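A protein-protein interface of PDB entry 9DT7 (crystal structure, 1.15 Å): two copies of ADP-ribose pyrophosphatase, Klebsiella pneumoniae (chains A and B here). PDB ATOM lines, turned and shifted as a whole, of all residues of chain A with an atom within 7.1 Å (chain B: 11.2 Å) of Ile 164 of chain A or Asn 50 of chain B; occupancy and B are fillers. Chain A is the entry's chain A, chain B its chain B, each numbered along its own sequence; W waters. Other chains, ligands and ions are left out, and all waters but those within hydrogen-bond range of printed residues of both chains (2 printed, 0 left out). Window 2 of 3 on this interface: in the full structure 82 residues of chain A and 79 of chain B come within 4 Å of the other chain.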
ATOM      1  N   GLU A 123     -11.104 -20.273 -38.824  1.00  0.00           N
ATOM      2  CA  GLU A 123     -10.819 -19.544 -37.585  1.00  0.00           C
ATOM      3  C   GLU A 123      -9.902 -20.323 -36.638  1.00  0.00           C
ATOM      4  O   GLU A 123      -9.077 -19.722 -35.933  1.00  0.00           O
ATOM      5  CB  GLU A 123     -12.130 -19.185 -36.869  1.00  0.00           C
ATOM      6  CG  GLU A 123     -13.026 -18.184 -37.624  1.00  0.00           C
ATOM      7  CD  GLU A 123     -14.273 -17.747 -36.827  1.00  0.00           C
ATOM      8  OE1 GLU A 123     -14.477 -18.235 -35.687  1.00  0.00           O
ATOM      9  OE2 GLU A 123     -15.047 -16.903 -37.344  1.00  0.00           O
ATOM     10  N   GLU A 124     -10.043 -21.648 -36.576  1.00  0.00           N
ATOM     11  CA  GLU A 124      -9.249 -22.444 -35.646  1.00  0.00           C
ATOM     12  C   GLU A 124      -7.940 -22.963 -36.218  1.00  0.00           C
ATOM     13  O   GLU A 124      -7.008 -23.228 -35.448  1.00  0.00           O
ATOM     14  CB  GLU A 124     -10.059 -23.635 -35.146  1.00  0.00           C
ATOM     15  CG  GLU A 124     -11.264 -23.204 -34.391  1.00  0.00           C
ATOM     16  CD  GLU A 124     -11.863 -24.300 -33.519  1.00  0.00           C
ATOM     17  OE1 GLU A 124     -11.761 -25.499 -33.851  1.00  0.00           O
ATOM     18  OE2 GLU A 124     -12.478 -23.963 -32.486  1.00  0.00           O
ATOM     19  N   LYS A 162      -0.645 -24.370 -40.678  1.00  0.00           N
ATOM     20  CA  LYS A 162       0.461 -23.931 -39.834  1.00  0.00           C
ATOM     21  C   LYS A 162      -0.032 -22.932 -38.798  1.00  0.00           C
ATOM     22  O   LYS A 162      -1.051 -22.266 -38.984  1.00  0.00           O
ATOM     23  CB  LYS A 162       1.556 -23.225 -40.663  1.00  0.00           C
ATOM     24  N   GLY A 163       0.721 -22.835 -37.710  1.00  0.00           N
ATOM     25  CA  GLY A 163       0.637 -21.667 -36.864  1.00  0.00           C
ATOM     26  C   GLY A 163      -0.243 -21.806 -35.641  1.00  0.00           C
ATOM     27  O   GLY A 163      -0.758 -22.877 -35.266  1.00  0.00           O
ATOM     28  N   ILE A 164      -0.377 -20.641 -34.977  1.00  0.00           N
ATOM     29  CA  ILE A 164      -1.142 -20.470 -33.747  1.00  0.00           C
ATOM     30  C   ILE A 164      -2.380 -19.652 -34.082  1.00  0.00           C
ATOM     31  O   ILE A 164      -2.293 -18.646 -34.803  1.00  0.00           O
ATOM     32  CB  ILE A 164      -0.297 -19.743 -32.675  1.00  0.00           C
ATOM     33  CG1 ILE A 164       0.909 -20.593 -32.262  1.00  0.00           C
ATOM     34  CG2 ILE A 164      -1.155 -19.386 -31.460  1.00  0.00           C
ATOM     35  CD1 ILE A 164       1.977 -19.827 -31.495  1.00  0.00           C
ATOM     36  N   HIS A 165      -3.535 -20.081 -33.560  1.00  0.00           N
ATOM     37  CA  HIS A 165      -4.815 -19.453 -33.859  1.00  0.00           C
ATOM     38  C   HIS A 165      -5.608 -19.273 -32.574  1.00  0.00           C
ATOM     39  O   HIS A 165      -5.143 -19.597 -31.480  1.00  0.00           O
ATOM     40  CB  HIS A 165      -5.562 -20.291 -34.905  1.00  0.00           C
ATOM     41  CG  HIS A 165      -4.793 -20.427 -36.174  1.00  0.00           C
ATOM     42  ND1 HIS A 165      -4.937 -19.552 -37.229  1.00  0.00           N
ATOM     43  CD2 HIS A 165      -3.822 -21.298 -36.535  1.00  0.00           C
ATOM     44  CE1 HIS A 165      -4.115 -19.904 -38.201  1.00  0.00           C
ATOM     45  NE2 HIS A 165      -3.421 -20.955 -37.799  1.00  0.00           N
ATOM     46  N   GLY A 166      -6.818 -18.754 -32.723  1.00  0.00           N
ATOM     47  CA  GLY A 166      -7.755 -18.569 -31.638  1.00  0.00           C
ATOM     48  C   GLY A 166      -8.004 -17.099 -31.333  1.00  0.00           C
ATOM     49  O   GLY A 166      -7.154 -16.230 -31.566  1.00  0.00           O
ATOM     50  N   GLU A 172      -8.530 -18.104 -26.129  1.00  0.00           N
ATOM     51  CA  GLU A 172      -8.464 -19.245 -27.033  1.00  0.00           C
ATOM     52  C   GLU A 172      -7.083 -19.280 -27.666  1.00  0.00           C
ATOM     53  O   GLU A 172      -6.700 -18.344 -28.382  1.00  0.00           O
ATOM     54  CB  GLU A 172      -9.535 -19.074 -28.109  1.00  0.00           C
ATOM     55  CG  GLU A 172      -9.928 -20.316 -28.867  1.00  0.00           C
ATOM     56  CD  GLU A 172     -11.052 -20.023 -29.847  1.00  0.00           C
ATOM     57  OE1 GLU A 172     -11.391 -18.827 -30.010  1.00  0.00           O
ATOM     58  OE2 GLU A 172     -11.592 -20.978 -30.449  1.00  0.00           O
ATOM     59  N   ASP A 173      -6.342 -20.358 -27.422  1.00  0.00           N
ATOM     60  CA  ASP A 173      -4.961 -20.501 -27.878  1.00  0.00           C
ATOM     61  C   ASP A 173      -4.826 -21.881 -28.513  1.00  0.00           C
ATOM     62  O   ASP A 173      -4.945 -22.902 -27.830  1.00  0.00           O
ATOM     63  CB  ASP A 173      -4.032 -20.337 -26.673  1.00  0.00           C
ATOM     64  CG  ASP A 173      -2.595 -20.305 -27.071  1.00  0.00           C
ATOM     65  OD1 ASP A 173      -2.284 -19.659 -28.084  1.00  0.00           O
ATOM     66  OD2 ASP A 173      -1.779 -20.920 -26.384  1.00  0.00           O
ATOM     67  N   ILE A 174      -4.588 -21.931 -29.828  1.00  0.00           N
ATOM     68  CA  ILE A 174      -4.699 -23.165 -30.599  1.00  0.00           C
ATOM     69  C   ILE A 174      -3.457 -23.330 -31.468  1.00  0.00           C
ATOM     70  O   ILE A 174      -3.015 -22.372 -32.105  1.00  0.00           O
ATOM     71  CB  ILE A 174      -5.974 -23.131 -31.467  1.00  0.00           C
ATOM     72  CG1 ILE A 174      -7.224 -22.829 -30.619  1.00  0.00           C
ATOM     73  CG2 ILE A 174      -6.161 -24.446 -32.219  1.00  0.00           C
ATOM     74  CD1 ILE A 174      -8.472 -22.681 -31.441  1.00  0.00           C
ATOM     75  N   ARG A 175      -2.898 -24.538 -31.496  1.00  0.00           N
ATOM     76  CA  ARG A 175      -1.756 -24.869 -32.339  1.00  0.00           C
ATOM     77  C   ARG A 175      -2.157 -25.935 -33.346  1.00  0.00           C
ATOM     78  O   ARG A 175      -2.826 -26.906 -33.016  1.00  0.00           O
ATOM     79  CB  ARG A 175      -0.596 -25.400 -31.480  1.00  0.00           C
ATOM     80  CG  ARG A 175       0.598 -25.807 -32.282  1.00  0.00           C
ATOM     81  CD  ARG A 175       1.768 -26.173 -31.399  1.00  0.00           C
ATOM     82  NE  ARG A 175       2.905 -26.553 -32.224  1.00  0.00           N
ATOM     83  CZ  ARG A 175       4.084 -26.938 -31.757  1.00  0.00           C
ATOM     84  NH1 ARG A 175       4.330 -26.964 -30.450  1.00  0.00           N
ATOM     85  NH2 ARG A 175       5.041 -27.293 -32.619  1.00  0.00           N
ATOM     86  N   VAL A 176      -1.703 -25.768 -34.576  1.00  0.00           N
ATOM     87  CA  VAL A 176      -2.047 -26.672 -35.676  1.00  0.00           C
ATOM     88  C   VAL A 176      -0.950 -27.718 -35.821  1.00  0.00           C
ATOM     89  O   VAL A 176       0.240 -27.396 -35.788  1.00  0.00           O
ATOM     90  CB  VAL A 176      -2.248 -25.865 -36.983  1.00  0.00           C
ATOM     91  CG1 VAL A 176      -2.337 -26.765 -38.205  1.00  0.00           C
ATOM     92  CG2 VAL A 176      -3.491 -25.007 -36.854  1.00  0.00           C
ATOM     93  N   THR B  18       2.064 -30.255 -26.742  1.00  0.00           N
ATOM     94  CA  THR B  18       3.150 -29.342 -26.446  1.00  0.00           C
ATOM     95  C   THR B  18       3.395 -29.183 -24.957  1.00  0.00           C
ATOM     96  O   THR B  18       4.541 -28.971 -24.546  1.00  0.00           O
ATOM     97  CB  THR B  18       2.793 -27.977 -27.044  1.00  0.00           C
ATOM     98  OG1 THR B  18       2.551 -28.109 -28.450  1.00  0.00           O
ATOM     99  CG2 THR B  18       3.909 -26.963 -26.852  1.00  0.00           C
ATOM    100  N   PHE B  19       2.348 -29.254 -24.131  1.00  0.00           N
ATOM    101  CA  PHE B  19       2.421 -28.879 -22.735  1.00  0.00           C
ATOM    102  C   PHE B  19       1.858 -29.999 -21.888  1.00  0.00           C
ATOM    103  O   PHE B  19       1.049 -30.816 -22.357  1.00  0.00           O
ATOM    104  CB  PHE B  19       1.625 -27.619 -22.523  1.00  0.00           C
ATOM    105  CG  PHE B  19       2.208 -26.399 -23.198  1.00  0.00           C
ATOM    106  CD1 PHE B  19       3.465 -25.927 -22.879  1.00  0.00           C
ATOM    107  CD2 PHE B  19       1.471 -25.695 -24.105  1.00  0.00           C
ATOM    108  CE1 PHE B  19       3.971 -24.787 -23.486  1.00  0.00           C
ATOM    109  CE2 PHE B  19       1.973 -24.533 -24.710  1.00  0.00           C
ATOM    110  CZ  PHE B  19       3.209 -24.103 -24.406  1.00  0.00           C
ATOM    111  N   HIS B  46      -2.460 -21.006 -17.530  1.00  0.00           N
ATOM    112  CA  HIS B  46      -1.743 -21.985 -18.321  1.00  0.00           C
ATOM    113  C   HIS B  46      -0.789 -21.307 -19.301  1.00  0.00           C
ATOM    114  O   HIS B  46      -0.992 -20.175 -19.730  1.00  0.00           O
ATOM    115  CB  HIS B  46      -2.721 -22.913 -19.084  1.00  0.00           C
ATOM    116  CG  HIS B  46      -3.557 -22.225 -20.118  1.00  0.00           C
ATOM    117  ND1 HIS B  46      -3.132 -22.006 -21.410  1.00  0.00           N
ATOM    118  CD2 HIS B  46      -4.783 -21.665 -20.020  1.00  0.00           C
ATOM    119  CE1 HIS B  46      -4.089 -21.370 -22.069  1.00  0.00           C
ATOM    120  NE2 HIS B  46      -5.106 -21.159 -21.252  1.00  0.00           N
ATOM    121  N   ARG B  47       0.228 -22.045 -19.695  1.00  0.00           N
ATOM    122  CA  ARG B  47       1.136 -21.576 -20.727  1.00  0.00           C
ATOM    123  C   ARG B  47       0.442 -21.432 -22.073  1.00  0.00           C
ATOM    124  O   ARG B  47      -0.461 -22.198 -22.431  1.00  0.00           O
ATOM    125  CB  ARG B  47       2.325 -22.528 -20.863  1.00  0.00           C
ATOM    126  CG  ARG B  47       3.305 -22.510 -19.701  1.00  0.00           C
ATOM    127  CD  ARG B  47       3.968 -21.146 -19.463  1.00  0.00           C
ATOM    128  NE  ARG B  47       4.882 -20.769 -20.518  1.00  0.00           N
ATOM    129  CZ  ARG B  47       6.172 -20.492 -20.344  1.00  0.00           C
ATOM    130  NH1 ARG B  47       6.748 -20.554 -19.138  1.00  0.00           N
ATOM    131  NH2 ARG B  47       6.900 -20.141 -21.398  1.00  0.00           N
ATOM    132  N   LEU B  48       0.943 -20.487 -22.856  1.00  0.00           N
ATOM    133  CA  LEU B  48       0.475 -20.157 -24.190  1.00  0.00           C
ATOM    134  C   LEU B  48       1.480 -20.615 -25.244  1.00  0.00           C
ATOM    135  O   LEU B  48       2.697 -20.605 -25.002  1.00  0.00           O
ATOM    136  CB  LEU B  48       0.305 -18.647 -24.316  1.00  0.00           C
ATOM    137  CG  LEU B  48      -0.654 -18.010 -23.327  1.00  0.00           C
ATOM    138  CD1 LEU B  48      -0.564 -16.482 -23.395  1.00  0.00           C
ATOM    139  CD2 LEU B  48      -2.074 -18.449 -23.602  1.00  0.00           C
ATOM    140  N   PHE B  49       0.963 -20.981 -26.427  1.00  0.00           N
ATOM    141  CA  PHE B  49       1.846 -21.414 -27.500  1.00  0.00           C
ATOM    142  C   PHE B  49       2.861 -20.343 -27.883  1.00  0.00           C
ATOM    143  O   PHE B  49       3.959 -20.692 -28.302  1.00  0.00           O
ATOM    144  CB  PHE B  49       1.030 -21.863 -28.707  1.00  0.00           C
ATOM    145  CG  PHE B  49       0.232 -23.093 -28.429  1.00  0.00           C
ATOM    146  CD1 PHE B  49       0.865 -24.285 -28.118  1.00  0.00           C
ATOM    147  CD2 PHE B  49      -1.141 -23.069 -28.446  1.00  0.00           C
ATOM    148  CE1 PHE B  49       0.133 -25.447 -27.860  1.00  0.00           C
ATOM    149  CE2 PHE B  49      -1.879 -24.210 -28.175  1.00  0.00           C
ATOM    150  CZ  PHE B  49      -1.231 -25.398 -27.864  1.00  0.00           C
ATOM    151  N   ASN B  50       2.542 -19.056 -27.705  1.00  0.00           N
ATOM    152  CA  ASN B  50       3.443 -17.973 -28.099  1.00  0.00           C
ATOM    153  C   ASN B  50       4.550 -17.715 -27.089  1.00  0.00           C
ATOM    154  O   ASN B  50       5.374 -16.826 -27.308  1.00  0.00           O
ATOM    155  CB  ASN B  50       2.672 -16.671 -28.363  1.00  0.00           C
ATOM    156  CG  ASN B  50       2.067 -16.048 -27.103  1.00  0.00           C
ATOM    157  OD1 ASN B  50       2.433 -16.363 -25.968  1.00  0.00           O
ATOM    158  ND2 ASN B  50       1.127 -15.132 -27.317  1.00  0.00           N
ATOM    159  N   GLY B  51       4.590 -18.447 -25.989  1.00  0.00           N
ATOM    160  CA  GLY B  51       5.676 -18.355 -25.047  1.00  0.00           C
ATOM    161  C   GLY B  51       5.295 -17.755 -23.718  1.00  0.00           C
ATOM    162  O   GLY B  51       6.081 -17.844 -22.767  1.00  0.00           O
ATOM    163  N   GLY B  52       4.142 -17.103 -23.618  1.00  0.00           N
ATOM    164  CA  GLY B  52       3.736 -16.483 -22.376  1.00  0.00           C
ATOM    165  C   GLY B  52       2.868 -17.370 -21.487  1.00  0.00           C
ATOM    166  O   GLY B  52       2.650 -18.564 -21.728  1.00  0.00           O
ATOM    167  N   MET B  53       2.343 -16.725 -20.457  1.00  0.00           N
ATOM    168  CA  MET B  53       1.358 -17.298 -19.555  1.00  0.00           C
ATOM    169  C   MET B  53       0.020 -16.585 -19.736  1.00  0.00           C
ATOM    170  O   MET B  53      -0.042 -15.360 -19.884  1.00  0.00           O
ATOM    171  CB  MET B  53       1.822 -17.111 -18.111  1.00  0.00           C
ATOM    172  CG  MET B  53       1.015 -17.903 -17.094  1.00  0.00           C
ATOM    173  SD  MET B  53       1.256 -19.687 -17.153  1.00  0.00           S
ATOM    174  CE  MET B  53       2.794 -19.802 -16.259  1.00  0.00           C
ATOM    175  N   SER B  54      -1.074 -17.343 -19.684  1.00  0.00           N
ATOM    176  CA  SER B  54      -2.397 -16.742 -19.661  1.00  0.00           C
ATOM    177  C   SER B  54      -2.625 -15.991 -18.353  1.00  0.00           C
ATOM    178  O   SER B  54      -1.947 -16.218 -17.350  1.00  0.00           O
ATOM    179  CB  SER B  54      -3.469 -17.841 -19.749  1.00  0.00           C
ATOM    180  OG  SER B  54      -3.601 -18.565 -18.524  1.00  0.00           O
ATOM    181  N   GLY B  55      -3.617 -15.115 -18.354  1.00  0.00           N
ATOM    182  CA  GLY B  55      -4.183 -14.666 -17.103  1.00  0.00           C
ATOM    183  C   GLY B  55      -4.976 -15.790 -16.447  1.00  0.00           C
ATOM    184  O   GLY B  55      -5.029 -16.924 -16.917  1.00  0.00           O
HETATM  185  O   HOH W   1      -1.991 -23.113 -24.641  1.00  0.00           O
HETATM  186  O   HOH W   2      -0.139 -18.143 -27.904  1.00  0.00           O
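The guanidinium group of Arg 175 of chain A lies within hydrogen-bond range of the side-chain hydroxyl of Thr 18 of chain B, at 2.9 Å.
The side-chain carboxylate (OD2) of Asp 173 of chain A is in hydrogen-bond range of the backbone NH (N) of Phe 49 of chain B.
The backbone NH (N) of His 165 of chain A sits at hydrogen-bond distance from the backbone carbonyl oxygen (O) of Ile 174 of chain A (2.8 Å).
The side-chain amide oxygen (OD1) of Asn 50 of chain B sits at hydrogen-bond distance from the backbone NH (N) of Gly 52 of chain B, at 3.0 Å.
Ile 164 of chain A touches Phe 49 of chain B (CD1 to CB, 3.6 Å).
N of Asn 50 of chain B touches CD1 of Ile 164 of chain A, 3.9 Å away.
CA of Leu 48 of chain B touches OD2 of Asp 173 of chain A (3.2 Å).
Ile 174 of chain A touches Phe 49 of chain B.
N of Arg 175 of chain A touches CE2 of Phe 49 of chain B, 3.5 Å away.
No residue of chain B comes within 4 Å of Lys 162 of chain A.
No residue of chain B comes within 4 Å of Gly 163 of chain A.
Of the printed residues of chain B, Ile 164 of chain A touches Phe 49 (3.6 Å) and Asn 50 (3.9 Å).
No residue of chain B comes within 4 Å of His 165 of chain A.
No residue of chain B comes within 4 Å of Gly 166 of chain A.
Asp 173 of chain A touches two residues of chain B.
Of the printed residues of chain B, Arg 175 of chain A touches Thr 18 and Phe 49.
Of the printed residues of chain A, Thr 18 of chain B touches Arg 175 (2.9 Å).
Of the printed residues of chain A, Phe 49 of chain B touches Ile 164 (3.6 Å), Asp 173 (2.7 Å), Ile 174 (3.8 Å) and Arg 175 (3.5 Å).
The nearest printed residue of chain B that does not touch Ile 164 of chain A is Gly 51 of chain B (6.2 Å).
The nearest printed residue of chain A that does not touch Asn 50 of chain B is Asp 173 of chain A (4.9 Å).
Printed residues of chain A that touch a printed residue of chain B: Ile 164, Asp 173, Ile 174 and Arg 175.
Along chain A the printed residues that touch a printed residue of chain B span positions 164 to 175.
Printed residues of chain B that touch a printed residue of chain A: Thr 18, Leu 48, Phe 49 and Asn 50.
Hydrophobic or aromatic side chains of chain B that line the printed part of chain A: Leu 48 and Phe 49.
Along chain B the printed residues that touch a printed residue of chain A span positions 18 to 50.
No position is printed for both chains.
Of the 7 pairs that touch across the chains among the printed residues, none has its exchanged pair printed and touching as well.
Water W2 lies within hydrogen-bond range of OD1 of Asp 173 of chain A (2.6 Å), N of Asn 50 of chain B (2.8 Å) and N of Phe 49 of chain B (3.4 Å).
Water W1 lies within hydrogen-bond range of OD2 of Asp 173 of chain A (2.8 Å) and O of Arg 47 of chain B (2.8 Å).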
